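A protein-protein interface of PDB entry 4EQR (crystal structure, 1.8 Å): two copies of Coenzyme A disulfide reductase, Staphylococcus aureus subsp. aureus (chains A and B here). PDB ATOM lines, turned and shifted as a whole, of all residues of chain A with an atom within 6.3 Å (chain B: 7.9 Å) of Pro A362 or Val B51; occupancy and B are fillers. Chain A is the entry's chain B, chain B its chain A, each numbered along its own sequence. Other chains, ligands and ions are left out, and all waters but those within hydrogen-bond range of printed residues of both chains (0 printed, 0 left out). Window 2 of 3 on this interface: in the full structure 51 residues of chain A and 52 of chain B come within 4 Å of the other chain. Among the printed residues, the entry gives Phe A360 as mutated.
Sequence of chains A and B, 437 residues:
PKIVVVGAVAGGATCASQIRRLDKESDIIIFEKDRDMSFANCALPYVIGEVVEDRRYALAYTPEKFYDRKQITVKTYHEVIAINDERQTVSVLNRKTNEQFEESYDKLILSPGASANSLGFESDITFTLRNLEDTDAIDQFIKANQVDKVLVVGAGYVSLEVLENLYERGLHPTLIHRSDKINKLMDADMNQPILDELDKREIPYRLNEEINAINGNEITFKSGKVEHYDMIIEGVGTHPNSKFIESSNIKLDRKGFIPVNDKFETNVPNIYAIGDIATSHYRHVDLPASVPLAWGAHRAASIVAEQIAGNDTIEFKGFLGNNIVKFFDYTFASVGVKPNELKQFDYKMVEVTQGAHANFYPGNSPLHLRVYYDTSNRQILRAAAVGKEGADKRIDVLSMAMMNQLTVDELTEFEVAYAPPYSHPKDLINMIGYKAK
Of the 17 printed residues of chain B, 6 touch a printed residue of chain A.
Pro A362 touches one residue of chain B. Of the printed residues of chain A, Val B51 touches Pro A362. Printed residues of chain A within 4 Å of Tyr B46: Tyr A361. Of the printed residues of chain B, Tyr A361 touches Tyr B46 (3.7 Å) and Lys B326 (3.6 Å). Of the printed residues of chain A, Tyr B57 touches Asn A359 and Phe A360. Glu A389 touches none of the printed residues of chain B. The nearest residue of chain B that does not touch Pro A362 is Val B52 (5.1 Å). The nearest residue of chain A that does not touch Val B51 is Tyr A361 (4.8 Å). The nearest printed residue of chain A that does not touch Ala B43 is Tyr A361 (6.5 Å).
Among the printed residues, merely in contact across the chains: Asn A359 with Tyr B57 (3.4 Å), Phe A360 with Ala B43 (3.2 Å), Phe A360 with Val B52 (3.4 Å), Phe A360 with Tyr B57 (3.2 Å), Tyr A361 with Tyr B46 (3.7 Å), Tyr A361 with Lys B326 (3.6 Å) and Pro A362 with Val B51 (3.3 Å).
The backbone carbonyl oxygen of Tyr B46 lies within hydrogen-bond range of the backbone NH of Val B51 (2.9 Å). N of Val B52 is in hydrogen-bond range of O of Tyr B46 (3.0 Å). The side-chain carboxylate of Glu B164 is in salt-bridge range of the side-chain amino group of Lys B326, 2.8 Å away. The backbone carbonyl oxygen (O) of Tyr A361 lies within hydrogen-bond range of a ring nitrogen (NE2) of His A357 (3.3 Å). The backbone carbonyl oxygen (O) of Pro A362 sits at hydrogen-bond distance from a ring nitrogen (NE2) of His A357, at 2.8 Å.
No position is printed for both chains. Of the 7 pairs that touch across the chains among the printed residues, none has its exchanged pair printed and touching as well.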
ATOM      1  N   HIS A 357       6.201  30.211   6.594  1.00  0.00           N
ATOM      2  CA  HIS A 357       5.767  30.289   7.986  1.00  0.00           C
ATOM      3  C   HIS A 357       6.042  28.954   8.663  1.00  0.00           C
ATOM      4  O   HIS A 357       6.724  28.101   8.092  1.00  0.00           O
ATOM      5  CB  HIS A 357       4.283  30.648   8.067  1.00  0.00           C
ATOM      6  CG  HIS A 357       3.387  29.687   7.351  1.00  0.00           C
ATOM      7  ND1 HIS A 357       2.524  30.073   6.350  1.00  0.00           N
ATOM      8  CD2 HIS A 357       3.207  28.350   7.502  1.00  0.00           C
ATOM      9  CE1 HIS A 357       1.860  29.020   5.905  1.00  0.00           C
ATOM     10  NE2 HIS A 357       2.258  27.964   6.591  1.00  0.00           N
ATOM     11  N   ALA A 358       5.504  28.764   9.865  1.00  0.00           N
ATOM     12  CA  ALA A 358       5.895  27.617  10.685  1.00  0.00           C
ATOM     13  C   ALA A 358       5.750  26.301   9.930  1.00  0.00           C
ATOM     14  O   ALA A 358       4.728  26.044   9.297  1.00  0.00           O
ATOM     15  CB  ALA A 358       5.101  27.579  11.989  1.00  0.00           C
ATOM     16  N   ASN A 359       6.788  25.475   9.999  1.00  0.00           N
ATOM     17  CA  ASN A 359       6.770  24.181   9.332  1.00  0.00           C
ATOM     18  C   ASN A 359       5.590  23.330   9.777  1.00  0.00           C
ATOM     19  O   ASN A 359       4.900  22.734   8.946  1.00  0.00           O
ATOM     20  CB  ASN A 359       8.092  23.447   9.557  1.00  0.00           C
ATOM     21  CG  ASN A 359       9.261  24.160   8.906  1.00  0.00           C
ATOM     22  OD1 ASN A 359       9.159  24.630   7.769  1.00  0.00           O
ATOM     23  ND2 ASN A 359      10.380  24.254   9.625  1.00  0.00           N
ATOM     24  N   PHE A 360       5.347  23.294  11.087  1.00  0.00           N
ATOM     25  CA  PHE A 360       4.212  22.547  11.624  1.00  0.00           C
ATOM     26  C   PHE A 360       2.872  23.172  11.238  1.00  0.00           C
ATOM     27  O   PHE A 360       1.824  22.546  11.392  1.00  0.00           O
ATOM     28  CB  PHE A 360       4.307  22.410  13.151  1.00  0.00           C
ATOM     29  CG  PHE A 360       4.337  23.728  13.883  1.00  0.00           C
ATOM     30  CD1 PHE A 360       3.204  24.526  13.951  1.00  0.00           C
ATOM     31  CD2 PHE A 360       5.499  24.165  14.502  1.00  0.00           C
ATOM     32  CE1 PHE A 360       3.229  25.739  14.620  1.00  0.00           C
ATOM     33  CE2 PHE A 360       5.535  25.392  15.172  1.00  0.00           C
ATOM     34  CZ  PHE A 360       4.402  26.172  15.234  1.00  0.00           C
ATOM     35  N   TYR A 361       2.911  24.409  10.746  1.00  0.00           N
ATOM     36  CA  TYR A 361       1.691  25.142  10.414  1.00  0.00           C
ATOM     37  C   TYR A 361       1.270  24.909   8.960  1.00  0.00           C
ATOM     38  O   TYR A 361       2.093  25.012   8.051  1.00  0.00           O
ATOM     39  CB  TYR A 361       1.880  26.638  10.685  1.00  0.00           C
ATOM     40  CG  TYR A 361       0.590  27.429  10.722  1.00  0.00           C
ATOM     41  CD1 TYR A 361      -0.119  27.577  11.903  1.00  0.00           C
ATOM     42  CD2 TYR A 361       0.084  28.023   9.579  1.00  0.00           C
ATOM     43  CE1 TYR A 361      -1.295  28.297  11.952  1.00  0.00           C
ATOM     44  CE2 TYR A 361      -1.095  28.748   9.617  1.00  0.00           C
ATOM     45  CZ  TYR A 361      -1.784  28.873  10.808  1.00  0.00           C
ATOM     46  OH  TYR A 361      -2.959  29.589  10.861  1.00  0.00           O
ATOM     47  N   PRO A 362      -0.024  24.620   8.739  1.00  0.00           N
ATOM     48  CA  PRO A 362      -0.588  24.220   7.444  1.00  0.00           C
ATOM     49  C   PRO A 362      -0.467  25.308   6.393  1.00  0.00           C
ATOM     50  O   PRO A 362      -0.071  26.427   6.711  1.00  0.00           O
ATOM     51  CB  PRO A 362      -2.072  23.996   7.758  1.00  0.00           C
ATOM     52  CG  PRO A 362      -2.154  23.859   9.232  1.00  0.00           C
ATOM     53  CD  PRO A 362      -1.062  24.720   9.776  1.00  0.00           C
ATOM     54  N   GLY A 363      -0.822  24.976   5.155  1.00  0.00           N
ATOM     55  CA  GLY A 363      -0.806  25.934   4.066  1.00  0.00           C
ATOM     56  C   GLY A 363       0.581  26.461   3.746  1.00  0.00           C
ATOM     57  O   GLY A 363       0.722  27.460   3.042  1.00  0.00           O
ATOM     58  N   ASN A 364       1.606  25.780   4.250  1.00  0.00           N
ATOM     59  CA  ASN A 364       2.985  26.228   4.069  1.00  0.00           C
ATOM     60  C   ASN A 364       3.508  25.999   2.649  1.00  0.00           C
ATOM     61  O   ASN A 364       3.069  25.089   1.948  1.00  0.00           O
ATOM     62  CB  ASN A 364       3.905  25.556   5.096  1.00  0.00           C
ATOM     63  CG  ASN A 364       5.119  26.416   5.464  1.00  0.00           C
ATOM     64  OD1 ASN A 364       5.209  27.594   5.100  1.00  0.00           O
ATOM     65  ND2 ASN A 364       6.051  25.826   6.201  1.00  0.00           N
ATOM     66  N   GLU A 389       4.250  32.238  -1.012  1.00  0.00           N
ATOM     67  CA  GLU A 389       3.930  33.062   0.144  1.00  0.00           C
ATOM     68  C   GLU A 389       5.158  33.781   0.726  1.00  0.00           C
ATOM     69  O   GLU A 389       6.247  33.213   0.806  1.00  0.00           O
ATOM     70  CB  GLU A 389       3.284  32.177   1.218  1.00  0.00           C
ATOM     71  CG  GLU A 389       3.105  32.838   2.571  1.00  0.00           C
ATOM     72  CD  GLU A 389       2.413  31.929   3.578  1.00  0.00           C
ATOM     73  OE1 GLU A 389       2.535  32.186   4.797  1.00  0.00           O
ATOM     74  OE2 GLU A 389       1.748  30.958   3.151  1.00  0.00           O
ATOM     75  N   ALA B  43       3.239  25.934  18.639  1.00  0.00           N
ATOM     76  CA  ALA B  43       2.288  25.098  17.916  1.00  0.00           C
ATOM     77  C   ALA B  43       1.160  24.589  18.811  1.00  0.00           C
ATOM     78  O   ALA B  43       0.130  24.126  18.319  1.00  0.00           O
ATOM     79  CB  ALA B  43       3.005  23.920  17.259  1.00  0.00           C
ATOM     80  N   PRO B  45      -1.373  25.657  20.716  1.00  0.00           N
ATOM     81  CA  PRO B  45      -2.794  25.991  20.551  1.00  0.00           C
ATOM     82  C   PRO B  45      -3.389  25.287  19.333  1.00  0.00           C
ATOM     83  O   PRO B  45      -4.555  24.891  19.340  1.00  0.00           O
ATOM     84  CB  PRO B  45      -2.776  27.518  20.344  1.00  0.00           C
ATOM     85  CG  PRO B  45      -1.517  27.964  21.057  1.00  0.00           C
ATOM     86  CD  PRO B  45      -0.526  26.864  20.746  1.00  0.00           C
ATOM     87  N   TYR B  46      -2.575  25.139  18.299  1.00  0.00           N
ATOM     88  CA  TYR B  46      -3.011  24.571  17.029  1.00  0.00           C
ATOM     89  C   TYR B  46      -3.077  23.051  17.101  1.00  0.00           C
ATOM     90  O   TYR B  46      -3.815  22.409  16.351  1.00  0.00           O
ATOM     91  CB  TYR B  46      -2.088  25.048  15.902  1.00  0.00           C
ATOM     92  CG  TYR B  46      -2.049  26.561  15.822  1.00  0.00           C
ATOM     93  CD1 TYR B  46      -1.007  27.279  16.399  1.00  0.00           C
ATOM     94  CD2 TYR B  46      -3.078  27.267  15.225  1.00  0.00           C
ATOM     95  CE1 TYR B  46      -0.974  28.661  16.349  1.00  0.00           C
ATOM     96  CE2 TYR B  46      -3.062  28.660  15.180  1.00  0.00           C
ATOM     97  CZ  TYR B  46      -2.002  29.346  15.739  1.00  0.00           C
ATOM     98  OH  TYR B  46      -1.978  30.722  15.704  1.00  0.00           O
ATOM     99  N   VAL B  47      -2.303  22.476  18.012  1.00  0.00           N
ATOM    100  CA  VAL B  47      -2.442  21.055  18.311  1.00  0.00           C
ATOM    101  C   VAL B  47      -3.803  20.835  18.963  1.00  0.00           C
ATOM    102  O   VAL B  47      -4.552  19.935  18.583  1.00  0.00           O
ATOM    103  CB  VAL B  47      -1.339  20.558  19.248  1.00  0.00           C
ATOM    104  CG1 VAL B  47      -1.623  19.125  19.674  1.00  0.00           C
ATOM    105  CG2 VAL B  47       0.035  20.674  18.571  1.00  0.00           C
ATOM    106  N   ILE B  48      -4.135  21.680  19.935  1.00  0.00           N
ATOM    107  CA  ILE B  48      -5.456  21.612  20.552  1.00  0.00           C
ATOM    108  C   ILE B  48      -6.578  21.756  19.522  1.00  0.00           C
ATOM    109  O   ILE B  48      -7.625  21.112  19.635  1.00  0.00           O
ATOM    110  CB  ILE B  48      -5.628  22.681  21.652  1.00  0.00           C
ATOM    111  CG1 ILE B  48      -4.721  22.356  22.850  1.00  0.00           C
ATOM    112  CG2 ILE B  48      -7.085  22.766  22.090  1.00  0.00           C
ATOM    113  CD1 ILE B  48      -4.727  23.419  23.946  1.00  0.00           C
ATOM    114  N   GLY B  49      -6.360  22.602  18.518  1.00  0.00           N
ATOM    115  CA  GLY B  49      -7.380  22.853  17.509  1.00  0.00           C
ATOM    116  C   GLY B  49      -7.420  21.794  16.419  1.00  0.00           C
ATOM    117  O   GLY B  49      -8.266  21.846  15.525  1.00  0.00           O
ATOM    118  N   GLU B  50      -6.500  20.839  16.495  1.00  0.00           N
ATOM    119  CA  GLU B  50      -6.412  19.766  15.507  1.00  0.00           C
ATOM    120  C   GLU B  50      -6.063  20.312  14.122  1.00  0.00           C
ATOM    121  O   GLU B  50      -6.303  19.667  13.107  1.00  0.00           O
ATOM    122  CB  GLU B  50      -7.702  18.936  15.491  1.00  0.00           C
ATOM    123  CG  GLU B  50      -8.022  18.332  16.858  1.00  0.00           C
ATOM    124  CD  GLU B  50      -9.305  17.519  16.887  1.00  0.00           C
ATOM    125  OE1 GLU B  50      -9.466  16.718  17.830  1.00  0.00           O
ATOM    126  OE2 GLU B  50     -10.149  17.675  15.984  1.00  0.00           O
ATOM    127  N   VAL B  51      -5.498  21.515  14.110  1.00  0.00           N
ATOM    128  CA  VAL B  51      -4.928  22.122  12.920  1.00  0.00           C
ATOM    129  C   VAL B  51      -3.568  21.470  12.678  1.00  0.00           C
ATOM    130  O   VAL B  51      -3.140  21.283  11.536  1.00  0.00           O
ATOM    131  CB  VAL B  51      -4.778  23.646  13.115  1.00  0.00           C
ATOM    132  CG1 VAL B  51      -3.791  24.236  12.125  1.00  0.00           C
ATOM    133  CG2 VAL B  51      -6.133  24.323  12.999  1.00  0.00           C
ATOM    134  N   VAL B  52      -2.902  21.120  13.775  1.00  0.00           N
ATOM    135  CA  VAL B  52      -1.681  20.327  13.749  1.00  0.00           C
ATOM    136  C   VAL B  52      -2.022  18.923  14.239  1.00  0.00           C
ATOM    137  O   VAL B  52      -2.094  18.674  15.445  1.00  0.00           O
ATOM    138  CB  VAL B  52      -0.595  20.907  14.688  1.00  0.00           C
ATOM    139  CG1 VAL B  52       0.567  19.923  14.828  1.00  0.00           C
ATOM    140  CG2 VAL B  52      -0.104  22.250  14.190  1.00  0.00           C
ATOM    141  N   GLU B  53      -2.236  18.005  13.304  1.00  0.00           N
ATOM    142  CA  GLU B  53      -2.628  16.643  13.646  1.00  0.00           C
ATOM    143  C   GLU B  53      -1.405  15.801  13.991  1.00  0.00           C
ATOM    144  O   GLU B  53      -1.388  15.087  14.996  1.00  0.00           O
ATOM    145  CB  GLU B  53      -3.381  16.002  12.476  1.00  0.00           C
ATOM    146  CG  GLU B  53      -4.639  16.746  12.039  1.00  0.00           C
ATOM    147  CD  GLU B  53      -5.892  16.260  12.756  1.00  0.00           C
ATOM    148  OE1 GLU B  53      -7.002  16.430  12.198  1.00  0.00           O
ATOM    149  OE2 GLU B  53      -5.766  15.703  13.867  1.00  0.00           O
ATOM    150  N   ASP B  54      -0.383  15.896  13.143  1.00  0.00           N
ATOM    151  CA  ASP B  54       0.836  15.104  13.286  1.00  0.00           C
ATOM    152  C   ASP B  54       1.636  15.532  14.514  1.00  0.00           C
ATOM    153  O   ASP B  54       2.359  16.525  14.470  1.00  0.00           O
ATOM    154  CB  ASP B  54       1.694  15.253  12.025  1.00  0.00           C
ATOM    155  CG  ASP B  54       2.764  14.181  11.909  1.00  0.00           C
ATOM    156  OD1 ASP B  54       3.417  14.110  10.844  1.00  0.00           O
ATOM    157  OD2 ASP B  54       2.951  13.408  12.871  1.00  0.00           O
ATOM    158  N   TYR B  57       4.922  16.993  14.568  1.00  0.00           N
ATOM    159  CA  TYR B  57       5.109  18.421  14.354  1.00  0.00           C
ATOM    160  C   TYR B  57       5.288  19.159  15.675  1.00  0.00           C
ATOM    161  O   TYR B  57       5.827  20.258  15.708  1.00  0.00           O
ATOM    162  CB  TYR B  57       3.898  19.012  13.631  1.00  0.00           C
ATOM    163  CG  TYR B  57       3.993  19.019  12.125  1.00  0.00           C
ATOM    164  CD1 TYR B  57       2.938  18.564  11.343  1.00  0.00           C
ATOM    165  CD2 TYR B  57       5.133  19.486  11.483  1.00  0.00           C
ATOM    166  CE1 TYR B  57       3.015  18.575   9.961  1.00  0.00           C
ATOM    167  CE2 TYR B  57       5.221  19.500  10.101  1.00  0.00           C
ATOM    168  CZ  TYR B  57       4.158  19.043   9.344  1.00  0.00           C
ATOM    169  OH  TYR B  57       4.240  19.054   7.965  1.00  0.00           O
ATOM    170  N   GLU B 164      -9.653  30.430  19.498  1.00  0.00           N
ATOM    171  CA  GLU B 164      -9.933  30.199  18.086  1.00  0.00           C
ATOM    172  C   GLU B 164      -9.857  28.712  17.772  1.00  0.00           C
ATOM    173  O   GLU B 164     -10.722  28.154  17.092  1.00  0.00           O
ATOM    174  CB  GLU B 164      -8.976  30.978  17.177  1.00  0.00           C
ATOM    175  CG  GLU B 164      -9.146  30.591  15.710  1.00  0.00           C
ATOM    176  CD  GLU B 164      -8.428  31.512  14.736  1.00  0.00           C
ATOM    177  OE1 GLU B 164      -7.677  32.408  15.173  1.00  0.00           O
ATOM    178  OE2 GLU B 164      -8.628  31.329  13.514  1.00  0.00           O
ATOM    179  N   ASN B 165      -8.812  28.069  18.275  1.00  0.00           N
ATOM    180  CA  ASN B 165      -8.640  26.640  18.044  1.00  0.00           C
ATOM    181  C   ASN B 165      -9.746  25.754  18.627  1.00  0.00           C
ATOM    182  O   ASN B 165     -10.168  24.783  17.989  1.00  0.00           O
ATOM    183  CB  ASN B 165      -7.250  26.196  18.493  1.00  0.00           C
ATOM    184  CG  ASN B 165      -6.208  26.458  17.426  1.00  0.00           C
ATOM    185  OD1 ASN B 165      -6.128  25.719  16.456  1.00  0.00           O
ATOM    186  ND2 ASN B 165      -5.434  27.536  17.581  1.00  0.00           N
ATOM    187  N   GLU B 168     -12.692  26.245  16.277  1.00  0.00           N
ATOM    188  CA  GLU B 168     -12.555  25.544  14.996  1.00  0.00           C
ATOM    189  C   GLU B 168     -12.604  24.013  15.154  1.00  0.00           C
ATOM    190  O   GLU B 168     -12.923  23.283  14.209  1.00  0.00           O
ATOM    191  CB  GLU B 168     -11.289  25.983  14.255  1.00  0.00           C
ATOM    192  CG  GLU B 168     -11.268  27.466  13.872  1.00  0.00           C
ATOM    193  CD  GLU B 168     -12.303  27.833  12.811  1.00  0.00           C
ATOM    194  OE1 GLU B 168     -12.447  29.035  12.499  1.00  0.00           O
ATOM    195  OE2 GLU B 168     -12.977  26.922  12.286  1.00  0.00           O
ATOM    196  N   ARG B 169     -12.299  23.535  16.353  1.00  0.00           N
ATOM    197  CA  ARG B 169     -12.379  22.108  16.646  1.00  0.00           C
ATOM    198  C   ARG B 169     -13.837  21.665  16.765  1.00  0.00           C
ATOM    199  O   ARG B 169     -14.147  20.470  16.682  1.00  0.00           O
ATOM    200  CB  ARG B 169     -11.611  21.788  17.933  1.00  0.00           C
ATOM    201  CG  ARG B 169     -11.663  20.318  18.368  1.00  0.00           C
ATOM    202  CD  ARG B 169     -10.595  20.028  19.416  1.00  0.00           C
ATOM    203  NE  ARG B 169     -10.757  18.706  20.022  1.00  0.00           N
ATOM    204  CZ  ARG B 169      -9.810  18.065  20.695  1.00  0.00           C
ATOM    205  NH1 ARG B 169      -8.616  18.616  20.851  1.00  0.00           N
ATOM    206  NH2 ARG B 169     -10.053  16.864  21.212  1.00  0.00           N
ATOM    207  N   LYS B 326      -2.431  36.156  15.002  1.00  0.00           N
ATOM    208  CA  LYS B 326      -3.577  35.973  14.125  1.00  0.00           C
ATOM    209  C   LYS B 326      -4.786  35.644  14.975  1.00  0.00           C
ATOM    210  O   LYS B 326      -4.703  34.811  15.880  1.00  0.00           O
ATOM    211  CB  LYS B 326      -3.316  34.840  13.127  1.00  0.00           C
ATOM    212  CG  LYS B 326      -4.576  34.305  12.450  1.00  0.00           C
ATOM    213  CD  LYS B 326      -4.318  32.947  11.790  1.00  0.00           C
ATOM    214  CE  LYS B 326      -5.430  31.940  12.092  1.00  0.00           C
ATOM    215  NZ  LYS B 326      -6.803  32.416  11.750  1.00  0.00           N
